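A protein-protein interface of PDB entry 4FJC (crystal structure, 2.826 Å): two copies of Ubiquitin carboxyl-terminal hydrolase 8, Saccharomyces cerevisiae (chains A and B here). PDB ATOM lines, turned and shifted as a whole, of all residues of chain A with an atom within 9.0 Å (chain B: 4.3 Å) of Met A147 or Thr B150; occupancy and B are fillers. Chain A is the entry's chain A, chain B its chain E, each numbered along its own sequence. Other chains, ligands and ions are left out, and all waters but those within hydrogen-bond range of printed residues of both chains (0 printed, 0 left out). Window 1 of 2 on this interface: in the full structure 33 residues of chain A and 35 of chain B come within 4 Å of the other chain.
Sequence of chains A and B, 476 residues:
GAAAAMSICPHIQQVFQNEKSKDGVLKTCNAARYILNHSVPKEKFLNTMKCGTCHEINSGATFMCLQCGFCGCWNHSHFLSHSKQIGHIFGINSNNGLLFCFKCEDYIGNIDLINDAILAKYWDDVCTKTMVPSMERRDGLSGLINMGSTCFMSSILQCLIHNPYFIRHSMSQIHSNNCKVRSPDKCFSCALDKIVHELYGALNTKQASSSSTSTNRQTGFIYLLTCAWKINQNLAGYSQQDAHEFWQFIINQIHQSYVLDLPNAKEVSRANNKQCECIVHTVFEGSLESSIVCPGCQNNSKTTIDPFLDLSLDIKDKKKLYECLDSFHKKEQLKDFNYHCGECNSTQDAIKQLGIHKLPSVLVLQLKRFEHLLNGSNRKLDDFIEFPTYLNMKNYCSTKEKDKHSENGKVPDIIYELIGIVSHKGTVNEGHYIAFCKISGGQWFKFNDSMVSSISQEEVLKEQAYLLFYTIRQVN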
ATOM      1  N   LEU A 144     -11.707 -29.177 -18.637  1.00  0.00           N
ATOM      2  CA  LEU A 144     -10.950 -28.745 -17.485  1.00  0.00           C
ATOM      3  C   LEU A 144      -9.636 -29.518 -17.461  1.00  0.00           C
ATOM      4  O   LEU A 144      -9.592 -30.727 -17.184  1.00  0.00           O
ATOM      5  CB  LEU A 144     -11.760 -28.938 -16.215  1.00  0.00           C
ATOM      6  CG  LEU A 144     -12.921 -27.954 -16.196  1.00  0.00           C
ATOM      7  CD1 LEU A 144     -13.943 -28.301 -15.121  1.00  0.00           C
ATOM      8  CD2 LEU A 144     -12.354 -26.550 -16.028  1.00  0.00           C
ATOM      9  N   ILE A 145      -8.576 -28.788 -17.810  1.00  0.00           N
ATOM     10  CA  ILE A 145      -7.228 -29.321 -17.915  1.00  0.00           C
ATOM     11  C   ILE A 145      -6.855 -29.884 -16.560  1.00  0.00           C
ATOM     12  O   ILE A 145      -6.561 -29.131 -15.623  1.00  0.00           O
ATOM     13  CB  ILE A 145      -6.221 -28.230 -18.361  1.00  0.00           C
ATOM     14  CG1 ILE A 145      -6.152 -28.154 -19.894  1.00  0.00           C
ATOM     15  CG2 ILE A 145      -4.831 -28.506 -17.812  1.00  0.00           C
ATOM     16  CD1 ILE A 145      -7.432 -27.722 -20.588  1.00  0.00           C
ATOM     17  N   ASN A 146      -6.895 -31.212 -16.467  1.00  0.00           N
ATOM     18  CA  ASN A 146      -6.575 -31.901 -15.232  1.00  0.00           C
ATOM     19  C   ASN A 146      -5.078 -32.008 -14.977  1.00  0.00           C
ATOM     20  O   ASN A 146      -4.278 -32.207 -15.894  1.00  0.00           O
ATOM     21  CB  ASN A 146      -7.247 -33.274 -15.174  1.00  0.00           C
ATOM     22  CG  ASN A 146      -8.641 -33.203 -14.575  1.00  0.00           C
ATOM     23  OD1 ASN A 146      -8.796 -32.898 -13.395  1.00  0.00           O
ATOM     24  ND2 ASN A 146      -9.663 -33.473 -15.388  1.00  0.00           N
ATOM     25  N   MET A 147      -4.731 -31.872 -13.703  1.00  0.00           N
ATOM     26  CA  MET A 147      -3.359 -31.749 -13.258  1.00  0.00           C
ATOM     27  C   MET A 147      -2.838 -33.135 -12.807  1.00  0.00           C
ATOM     28  O   MET A 147      -2.613 -33.397 -11.603  1.00  0.00           O
ATOM     29  CB  MET A 147      -3.272 -30.704 -12.127  1.00  0.00           C
ATOM     30  CG  MET A 147      -4.039 -29.389 -12.363  1.00  0.00           C
ATOM     31  SD  MET A 147      -3.371 -28.335 -13.673  1.00  0.00           S
ATOM     32  CE  MET A 147      -3.463 -26.711 -12.928  1.00  0.00           C
ATOM     33  N   GLY A 148      -2.662 -34.021 -13.792  1.00  0.00           N
ATOM     34  CA  GLY A 148      -2.144 -35.370 -13.558  1.00  0.00           C
ATOM     35  C   GLY A 148      -0.710 -35.388 -13.046  1.00  0.00           C
ATOM     36  O   GLY A 148      -0.489 -35.555 -11.832  1.00  0.00           O
ATOM     37  N   SER A 149       0.251 -35.197 -13.968  1.00  0.00           N
ATOM     38  CA  SER A 149       1.699 -35.359 -13.684  1.00  0.00           C
ATOM     39  C   SER A 149       2.459 -34.052 -13.382  1.00  0.00           C
ATOM     40  O   SER A 149       2.594 -33.183 -14.230  1.00  0.00           O
ATOM     41  CB  SER A 149       2.394 -36.109 -14.836  1.00  0.00           C
ATOM     42  OG  SER A 149       2.255 -35.410 -16.066  1.00  0.00           O
ATOM     43  N   THR A 150       2.945 -33.947 -12.146  1.00  0.00           N
ATOM     44  CA  THR A 150       3.806 -32.853 -11.687  1.00  0.00           C
ATOM     45  C   THR A 150       5.189 -33.422 -11.357  1.00  0.00           C
ATOM     46  O   THR A 150       5.909 -32.894 -10.502  1.00  0.00           O
ATOM     47  CB  THR A 150       3.266 -32.199 -10.387  1.00  0.00           C
ATOM     48  OG1 THR A 150       3.470 -33.086  -9.275  1.00  0.00           O
ATOM     49  CG2 THR A 150       1.775 -31.846 -10.498  1.00  0.00           C
ATOM     50  N   CYS A 151       5.559 -34.510 -12.019  1.00  0.00           N
ATOM     51  CA  CYS A 151       6.762 -35.215 -11.661  1.00  0.00           C
ATOM     52  C   CYS A 151       7.938 -34.540 -12.349  1.00  0.00           C
ATOM     53  O   CYS A 151       9.099 -34.800 -12.011  1.00  0.00           O
ATOM     54  CB  CYS A 151       6.643 -36.679 -12.048  1.00  0.00           C
ATOM     55  SG  CYS A 151       6.875 -36.987 -13.800  1.00  0.00           S
ATOM     56  N   PHE A 152       7.635 -33.664 -13.303  1.00  0.00           N
ATOM     57  CA  PHE A 152       8.638 -32.746 -13.844  1.00  0.00           C
ATOM     58  C   PHE A 152       8.985 -31.612 -12.880  1.00  0.00           C
ATOM     59  O   PHE A 152       9.815 -30.787 -13.208  1.00  0.00           O
ATOM     60  CB  PHE A 152       8.153 -32.113 -15.154  1.00  0.00           C
ATOM     61  CG  PHE A 152       7.195 -30.968 -14.958  1.00  0.00           C
ATOM     62  CD1 PHE A 152       5.876 -31.201 -14.621  1.00  0.00           C
ATOM     63  CD2 PHE A 152       7.619 -29.660 -15.108  1.00  0.00           C
ATOM     64  CE1 PHE A 152       4.999 -30.152 -14.441  1.00  0.00           C
ATOM     65  CE2 PHE A 152       6.746 -28.602 -14.932  1.00  0.00           C
ATOM     66  CZ  PHE A 152       5.434 -28.848 -14.596  1.00  0.00           C
ATOM     67  N   LEU A 225       3.659 -25.619  -5.489  1.00  0.00           N
ATOM     68  CA  LEU A 225       2.833 -25.950  -6.630  1.00  0.00           C
ATOM     69  C   LEU A 225       1.929 -24.782  -7.036  1.00  0.00           C
ATOM     70  O   LEU A 225       1.897 -24.393  -8.200  1.00  0.00           O
ATOM     71  CB  LEU A 225       1.973 -27.189  -6.323  1.00  0.00           C
ATOM     72  CG  LEU A 225       2.247 -28.432  -7.167  1.00  0.00           C
ATOM     73  CD1 LEU A 225       1.315 -29.571  -6.754  1.00  0.00           C
ATOM     74  CD2 LEU A 225       2.080 -28.095  -8.653  1.00  0.00           C
ATOM     75  N   THR A 226       1.224 -24.226  -6.053  1.00  0.00           N
ATOM     76  CA  THR A 226       0.140 -23.281  -6.293  1.00  0.00           C
ATOM     77  C   THR A 226       0.644 -21.919  -6.760  1.00  0.00           C
ATOM     78  O   THR A 226       0.078 -21.343  -7.696  1.00  0.00           O
ATOM     79  CB  THR A 226      -0.755 -23.127  -5.041  1.00  0.00           C
ATOM     80  OG1 THR A 226       0.001 -22.588  -3.956  1.00  0.00           O
ATOM     81  CG2 THR A 226      -1.307 -24.479  -4.622  1.00  0.00           C
ATOM     82  N   ALA A 228       3.181 -21.507  -8.384  1.00  0.00           N
ATOM     83  CA  ALA A 228       3.601 -21.801  -9.743  1.00  0.00           C
ATOM     84  C   ALA A 228       2.497 -21.481 -10.730  1.00  0.00           C
ATOM     85  O   ALA A 228       2.708 -20.718 -11.669  1.00  0.00           O
ATOM     86  CB  ALA A 228       4.005 -23.269  -9.864  1.00  0.00           C
ATOM     87  N   TRP A 229       1.318 -22.058 -10.490  1.00  0.00           N
ATOM     88  CA  TRP A 229       0.209 -22.001 -11.441  1.00  0.00           C
ATOM     89  C   TRP A 229      -0.474 -20.688 -11.482  1.00  0.00           C
ATOM     90  O   TRP A 229      -1.207 -20.414 -12.421  1.00  0.00           O
ATOM     91  CB  TRP A 229      -0.834 -23.057 -11.143  1.00  0.00           C
ATOM     92  CG  TRP A 229      -0.330 -24.472 -11.215  1.00  0.00           C
ATOM     93  CD1 TRP A 229       0.871 -24.932 -11.754  1.00  0.00           C
ATOM     94  CD2 TRP A 229      -1.029 -25.681 -10.762  1.00  0.00           C
ATOM     95  NE1 TRP A 229       0.963 -26.300 -11.652  1.00  0.00           N
ATOM     96  CE2 TRP A 229      -0.141 -26.809 -11.065  1.00  0.00           C
ATOM     97  CE3 TRP A 229      -2.253 -25.928 -10.151  1.00  0.00           C
ATOM     98  CZ2 TRP A 229      -0.485 -28.111 -10.758  1.00  0.00           C
ATOM     99  CZ3 TRP A 229      -2.590 -27.244  -9.849  1.00  0.00           C
ATOM    100  CH2 TRP A 229      -1.724 -28.311 -10.142  1.00  0.00           C
ATOM    101  N   LYS A 230      -0.276 -19.875 -10.455  1.00  0.00           N
ATOM    102  CA  LYS A 230      -0.837 -18.543 -10.446  1.00  0.00           C
ATOM    103  C   LYS A 230       0.083 -17.579 -11.183  1.00  0.00           C
ATOM    104  O   LYS A 230      -0.320 -16.967 -12.184  1.00  0.00           O
ATOM    105  CB  LYS A 230      -1.078 -18.082  -9.013  1.00  0.00           C
ATOM    106  CG  LYS A 230      -2.167 -18.885  -8.315  1.00  0.00           C
ATOM    107  CD  LYS A 230      -2.212 -18.571  -6.831  1.00  0.00           C
ATOM    108  CE  LYS A 230      -3.250 -19.411  -6.114  1.00  0.00           C
ATOM    109  NZ  LYS A 230      -3.310 -19.026  -4.676  1.00  0.00           N
ATOM    110  N   ASN A 232       2.386 -18.120 -13.106  1.00  0.00           N
ATOM    111  CA  ASN A 232       2.499 -18.521 -14.497  1.00  0.00           C
ATOM    112  C   ASN A 232       1.150 -18.991 -15.035  1.00  0.00           C
ATOM    113  O   ASN A 232       0.779 -20.157 -14.883  1.00  0.00           O
ATOM    114  CB  ASN A 232       3.573 -19.599 -14.655  1.00  0.00           C
ATOM    115  CG  ASN A 232       4.404 -19.405 -15.911  1.00  0.00           C
ATOM    116  OD1 ASN A 232       3.916 -18.884 -16.917  1.00  0.00           O
ATOM    117  ND2 ASN A 232       5.667 -19.814 -15.857  1.00  0.00           N
ATOM    118  N   ASN A 234      -1.870 -19.633 -17.941  1.00  0.00           N
ATOM    119  CA  ASN A 234      -2.367 -20.647 -17.004  1.00  0.00           C
ATOM    120  C   ASN A 234      -1.222 -21.629 -16.717  1.00  0.00           C
ATOM    121  O   ASN A 234      -1.067 -22.099 -15.594  1.00  0.00           O
ATOM    122  CB  ASN A 234      -3.591 -21.377 -17.593  1.00  0.00           C
ATOM    123  CG  ASN A 234      -4.751 -20.430 -17.916  1.00  0.00           C
ATOM    124  OD1 ASN A 234      -5.560 -20.695 -18.809  1.00  0.00           O
ATOM    125  ND2 ASN A 234      -4.834 -19.323 -17.189  1.00  0.00           N
ATOM    126  N   LEU A 235      -0.413 -21.893 -17.746  1.00  0.00           N
ATOM    127  CA  LEU A 235       0.776 -22.744 -17.655  1.00  0.00           C
ATOM    128  C   LEU A 235       1.968 -21.811 -17.364  1.00  0.00           C
ATOM    129  O   LEU A 235       1.928 -20.660 -17.793  1.00  0.00           O
ATOM    130  CB  LEU A 235       1.016 -23.523 -18.968  1.00  0.00           C
ATOM    131  CG  LEU A 235      -0.051 -23.670 -20.078  1.00  0.00           C
ATOM    132  CD1 LEU A 235      -1.470 -23.839 -19.553  1.00  0.00           C
ATOM    133  CD2 LEU A 235       0.020 -22.516 -21.074  1.00  0.00           C
ATOM    134  N   ALA A 236       3.029 -22.255 -16.674  1.00  0.00           N
ATOM    135  CA  ALA A 236       3.227 -23.623 -16.167  1.00  0.00           C
ATOM    136  C   ALA A 236       2.085 -24.083 -15.259  1.00  0.00           C
ATOM    137  O   ALA A 236       1.475 -23.252 -14.588  1.00  0.00           O
ATOM    138  CB  ALA A 236       4.558 -23.717 -15.415  1.00  0.00           C
ATOM    139  N   GLY A 237       1.788 -25.387 -15.227  1.00  0.00           N
ATOM    140  CA  GLY A 237       2.566 -26.430 -15.909  1.00  0.00           C
ATOM    141  C   GLY A 237       1.989 -27.048 -17.180  1.00  0.00           C
ATOM    142  O   GLY A 237       2.704 -27.214 -18.171  1.00  0.00           O
ATOM    143  N   TYR A 238       0.692 -27.345 -17.176  1.00  0.00           N
ATOM    144  CA  TYR A 238       0.139 -28.494 -17.942  1.00  0.00           C
ATOM    145  C   TYR A 238      -0.023 -28.451 -19.494  1.00  0.00           C
ATOM    146  O   TYR A 238      -0.918 -29.093 -20.048  1.00  0.00           O
ATOM    147  CB  TYR A 238      -1.146 -28.978 -17.243  1.00  0.00           C
ATOM    148  CG  TYR A 238      -0.786 -29.839 -16.056  1.00  0.00           C
ATOM    149  CD1 TYR A 238      -0.179 -29.283 -14.925  1.00  0.00           C
ATOM    150  CD2 TYR A 238      -0.977 -31.221 -16.092  1.00  0.00           C
ATOM    151  CE1 TYR A 238       0.184 -30.070 -13.853  1.00  0.00           C
ATOM    152  CE2 TYR A 238      -0.611 -32.016 -15.025  1.00  0.00           C
ATOM    153  CZ  TYR A 238      -0.037 -31.433 -13.911  1.00  0.00           C
ATOM    154  OH  TYR A 238       0.318 -32.222 -12.851  1.00  0.00           O
ATOM    155  N   SER A 239       0.872 -27.740 -20.176  1.00  0.00           N
ATOM    156  CA  SER A 239       1.015 -27.838 -21.636  1.00  0.00           C
ATOM    157  C   SER A 239       2.288 -28.623 -21.984  1.00  0.00           C
ATOM    158  O   SER A 239       2.261 -29.571 -22.776  1.00  0.00           O
ATOM    159  CB  SER A 239       1.077 -26.438 -22.269  1.00  0.00           C
ATOM    160  OG  SER A 239       2.044 -25.610 -21.625  1.00  0.00           O
ATOM    161  N   GLN A 241       5.835 -30.057 -19.912  1.00  0.00           N
ATOM    162  CA  GLN A 241       6.485 -30.321 -18.649  1.00  0.00           C
ATOM    163  C   GLN A 241       7.955 -30.506 -18.957  1.00  0.00           C
ATOM    164  O   GLN A 241       8.480 -31.616 -18.890  1.00  0.00           O
ATOM    165  CB  GLN A 241       5.934 -31.606 -18.020  1.00  0.00           C
ATOM    166  CG  GLN A 241       4.476 -31.932 -18.308  1.00  0.00           C
ATOM    167  CD  GLN A 241       3.563 -30.814 -17.887  1.00  0.00           C
ATOM    168  OE1 GLN A 241       3.759 -29.661 -18.280  1.00  0.00           O
ATOM    169  NE2 GLN A 241       2.563 -31.140 -17.080  1.00  0.00           N
ATOM    170  N   SER B 149      -4.514 -38.145 -10.105  1.00  0.00           N
ATOM    171  CA  SER B 149      -5.260 -37.257 -10.991  1.00  0.00           C
ATOM    172  C   SER B 149      -6.109 -36.277 -10.181  1.00  0.00           C
ATOM    173  O   SER B 149      -6.415 -36.517  -9.006  1.00  0.00           O
ATOM    174  CB  SER B 149      -6.171 -38.080 -11.928  1.00  0.00           C
ATOM    175  OG  SER B 149      -6.812 -37.279 -12.923  1.00  0.00           O
ATOM    176  N   THR B 150      -6.480 -35.173 -10.828  1.00  0.00           N
ATOM    177  CA  THR B 150      -7.552 -34.299 -10.345  1.00  0.00           C
ATOM    178  C   THR B 150      -8.898 -34.561 -11.037  1.00  0.00           C
ATOM    179  O   THR B 150      -9.864 -33.835 -10.803  1.00  0.00           O
ATOM    180  CB  THR B 150      -7.181 -32.823 -10.538  1.00  0.00           C
ATOM    181  OG1 THR B 150      -6.503 -32.662 -11.793  1.00  0.00           O
ATOM    182  CG2 THR B 150      -6.301 -32.353  -9.381  1.00  0.00           C
ATOM    183  N   CYS B 151      -8.969 -35.603 -11.869  1.00  0.00           N
ATOM    184  CA  CYS B 151     -10.198 -35.913 -12.610  1.00  0.00           C
ATOM    185  C   CYS B 151     -11.377 -36.158 -11.671  1.00  0.00           C
ATOM    186  O   CYS B 151     -12.513 -36.006 -12.073  1.00  0.00           O
ATOM    187  CB  CYS B 151     -10.001 -37.092 -13.563  1.00  0.00           C
ATOM    188  SG  CYS B 151      -9.716 -38.680 -12.750  1.00  0.00           S
ATOM    189  N   PHE B 152     -11.113 -36.510 -10.416  1.00  0.00           N
ATOM    190  CA  PHE B 152     -12.190 -36.654  -9.431  1.00  0.00           C
ATOM    191  C   PHE B 152     -12.742 -35.321  -8.914  1.00  0.00           C
ATOM    192  O   PHE B 152     -13.732 -35.308  -8.208  1.00  0.00           O
ATOM    193  CB  PHE B 152     -11.736 -37.528  -8.247  1.00  0.00           C
ATOM    194  CG  PHE B 152     -11.014 -36.774  -7.171  1.00  0.00           C
ATOM    195  CD1 PHE B 152      -9.662 -36.520  -7.278  1.00  0.00           C
ATOM    196  CD2 PHE B 152     -11.698 -36.314  -6.047  1.00  0.00           C
ATOM    197  CE1 PHE B 152      -9.004 -35.815  -6.286  1.00  0.00           C
ATOM    198  CE2 PHE B 152     -11.043 -35.619  -5.048  1.00  0.00           C
ATOM    199  CZ  PHE B 152      -9.697 -35.364  -5.175  1.00  0.00           C
ATOM    200  N   MET B 153     -12.097 -34.205  -9.233  1.00  0.00           N
ATOM    201  CA  MET B 153     -12.634 -32.877  -8.874  1.00  0.00           C
ATOM    202  C   MET B 153     -13.261 -32.183 -10.072  1.00  0.00           C
ATOM    203  O   MET B 153     -14.235 -31.476  -9.922  1.00  0.00           O
ATOM    204  CB  MET B 153     -11.544 -31.999  -8.298  1.00  0.00           C
ATOM    205  CG  MET B 153     -10.798 -32.666  -7.164  1.00  0.00           C
ATOM    206  SD  MET B 153      -9.279 -31.812  -6.728  1.00  0.00           S
ATOM    207  CE  MET B 153      -9.948 -30.278  -6.093  1.00  0.00           C
ATOM    208  N   SER B 154     -12.707 -32.400 -11.259  1.00  0.00           N
ATOM    209  CA  SER B 154     -13.241 -31.793 -12.466  1.00  0.00           C
ATOM    210  C   SER B 154     -14.607 -32.389 -12.785  1.00  0.00           C
ATOM    211  O   SER B 154     -15.573 -31.676 -13.004  1.00  0.00           O
ATOM    212  CB  SER B 154     -12.272 -32.004 -13.629  1.00  0.00           C
ATOM    213  OG  SER B 154     -11.947 -33.375 -13.751  1.00  0.00           O
ATOM    214  N   ILE B 222      -7.921 -23.995 -11.677  1.00  0.00           N
ATOM    215  CA  ILE B 222      -6.665 -23.814 -10.957  1.00  0.00           C
ATOM    216  C   ILE B 222      -6.883 -23.141  -9.605  1.00  0.00           C
ATOM    217  O   ILE B 222      -6.607 -23.737  -8.557  1.00  0.00           O
ATOM    218  CB  ILE B 222      -5.692 -22.962 -11.789  1.00  0.00           C
ATOM    219  CG1 ILE B 222      -5.137 -23.779 -12.970  1.00  0.00           C
ATOM    220  CG2 ILE B 222      -4.564 -22.420 -10.911  1.00  0.00           C
ATOM    221  CD1 ILE B 222      -4.787 -22.938 -14.183  1.00  0.00           C
ATOM    222  N   LEU B 225      -8.876 -25.431  -7.402  1.00  0.00           N
ATOM    223  CA  LEU B 225      -8.041 -26.464  -6.820  1.00  0.00           C
ATOM    224  C   LEU B 225      -7.204 -25.890  -5.678  1.00  0.00           C
ATOM    225  O   LEU B 225      -7.168 -26.453  -4.583  1.00  0.00           O
ATOM    226  CB  LEU B 225      -7.091 -27.076  -7.848  1.00  0.00           C
ATOM    227  CG  LEU B 225      -7.655 -27.922  -8.986  1.00  0.00           C
ATOM    228  CD1 LEU B 225      -6.494 -28.692  -9.613  1.00  0.00           C
ATOM    229  CD2 LEU B 225      -8.761 -28.865  -8.506  1.00  0.00           C
ATOM    230  N   TRP B 229      -6.749 -27.369  -1.697  1.00  0.00           N
ATOM    231  CA  TRP B 229      -5.565 -27.901  -0.998  1.00  0.00           C
ATOM    232  C   TRP B 229      -5.155 -27.140   0.231  1.00  0.00           C
ATOM    233  O   TRP B 229      -4.820 -27.763   1.238  1.00  0.00           O
ATOM    234  CB  TRP B 229      -4.376 -27.950  -1.928  1.00  0.00           C
ATOM    235  CG  TRP B 229      -4.526 -28.920  -3.056  1.00  0.00           C
ATOM    236  CD1 TRP B 229      -5.011 -30.211  -2.997  1.00  0.00           C
ATOM    237  CD2 TRP B 229      -4.150 -28.724  -4.447  1.00  0.00           C
ATOM    238  NE1 TRP B 229      -4.976 -30.802  -4.228  1.00  0.00           N
ATOM    239  CE2 TRP B 229      -4.470 -29.970  -5.133  1.00  0.00           C
ATOM    240  CE3 TRP B 229      -3.606 -27.678  -5.169  1.00  0.00           C
ATOM    241  CZ2 TRP B 229      -4.255 -30.140  -6.473  1.00  0.00           C
ATOM    242  CZ3 TRP B 229      -3.389 -27.859  -6.531  1.00  0.00           C
ATOM    243  CH2 TRP B 229      -3.713 -29.064  -7.167  1.00  0.00           C
ATOM    244  N   TYR B 238      -5.174 -34.267  -2.102  1.00  0.00           N
ATOM    245  CA  TYR B 238      -5.259 -34.872  -3.429  1.00  0.00           C
ATOM    246  C   TYR B 238      -6.107 -36.137  -3.361  1.00  0.00           C
ATOM    247  O   TYR B 238      -6.467 -36.717  -4.389  1.00  0.00           O
ATOM    248  CB  TYR B 238      -3.841 -35.248  -3.880  1.00  0.00           C
ATOM    249  CG  TYR B 238      -3.661 -35.497  -5.354  1.00  0.00           C
ATOM    250  CD1 TYR B 238      -4.235 -34.648  -6.298  1.00  0.00           C
ATOM    251  CD2 TYR B 238      -2.869 -36.546  -5.808  1.00  0.00           C
ATOM    252  CE1 TYR B 238      -4.051 -34.856  -7.651  1.00  0.00           C
ATOM    253  CE2 TYR B 238      -2.679 -36.762  -7.161  1.00  0.00           C
ATOM    254  CZ  TYR B 238      -3.273 -35.913  -8.078  1.00  0.00           C
ATOM    255  OH  TYR B 238      -3.098 -36.096  -9.430  1.00  0.00           O
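The side-chain amide oxygen (OD1) of Asn A146 lies within hydrogen-bond range of the side-chain hydroxyl (OG1) of Thr B150 (2.8 Å).
The backbone NH (N) of Cys B151 is in hydrogen-bond range of the side-chain amide oxygen (OD1) of Asn A146 (3.1 Å).
The side-chain hydroxyl of Ser B154 is in hydrogen-bond range of the side-chain amide nitrogen of Asn A146, at 2.8 Å.
N of Met A147 lies within hydrogen-bond range of OG1 of Thr B150 (2.7 Å).
The backbone carbonyl oxygen (O) of Met A147 lies within hydrogen-bond range of the side-chain hydroxyl (OH) of Tyr B238, 3.5 Å away.
The backbone carbonyl oxygen (O) of Leu A144 is in hydrogen-bond range of the side-chain amide nitrogen (ND2) of Asn A146 (3.3 Å).
O of Met A147 sits close to OH of Tyr A238, 3.4 Å away.
OG of Ser B149 sits at hydrogen-bond distance from N of Cys B151, at 2.9 Å.
N of Ser B149 lies within hydrogen-bond range of OH of Tyr B238.
The backbone carbonyl oxygen of Cys B151 is in hydrogen-bond range of the side-chain hydroxyl of Ser B154.
Met A147 touches Ile B222.
Met A147 touches Leu B225 (CG to CD1, 3.8 Å).
Gly A148 touches Tyr B238 (O to OH, 3.6 Å).
Thr A226 touches Trp B229 (CG2 to CE3, 3.98 Å).
Trp A229 touches Ile B222.
Trp A229 touches Trp B229.
Ile B222 touches Asn A234.
Met A147 touches four residues of chain B.
Printed residues of chain B within 4 Å of Gly A148: Tyr B238.
Of the printed residues of chain B, Trp A229 touches Ile B222 (3.8 Å) and Trp B229 (3.4 Å).
Ala A236 touches none of the printed residues of chain B.
Gln A241 touches none of the printed residues of chain B.
Of chain A, only Asn A146 and Met A147 come within 4 Å of Thr B150.
Cys B151 touches just one residue of chain A: Asn A146 (3.1 Å).
Of the printed residues of chain A, Ser B154 touches Asn A146 (2.8 Å).
Of the printed residues of chain A, Leu B225 touches Met A147 (3.8 Å).
The nearest printed residue of chain B that does not touch Met A147 is Ser B149 (4.7 Å).
The nearest residue of chain A that does not touch Thr B150 is Gly A148 (4.5 Å).
Printed residues of chain B that touch a printed residue of chain A: Thr B150, Cys B151, Ser B154, Ile B222, Leu B225, Trp B229 and Tyr B238.
Hydrophobic or aromatic side chains of chain B that line the printed part of chain A: Ile B222, Leu B225, Trp B229 and Tyr B238.
Of the 22 printed residues of chain A, 6 touch a printed residue of chain B.
Printed residues of chain A that touch a printed residue of chain B: Asn A146, Met A147, Gly A148, Thr A226, Trp A229 and Asn A234.
Among the printed residues, 12 pairs touch across the chains.
Trp B229 touches its own counterpart, Trp A229.
7 positions are printed for both chains.
Of the 12 pairs that touch across the chains among the printed residues, 1 has its exchanged pair printed and touching as well.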
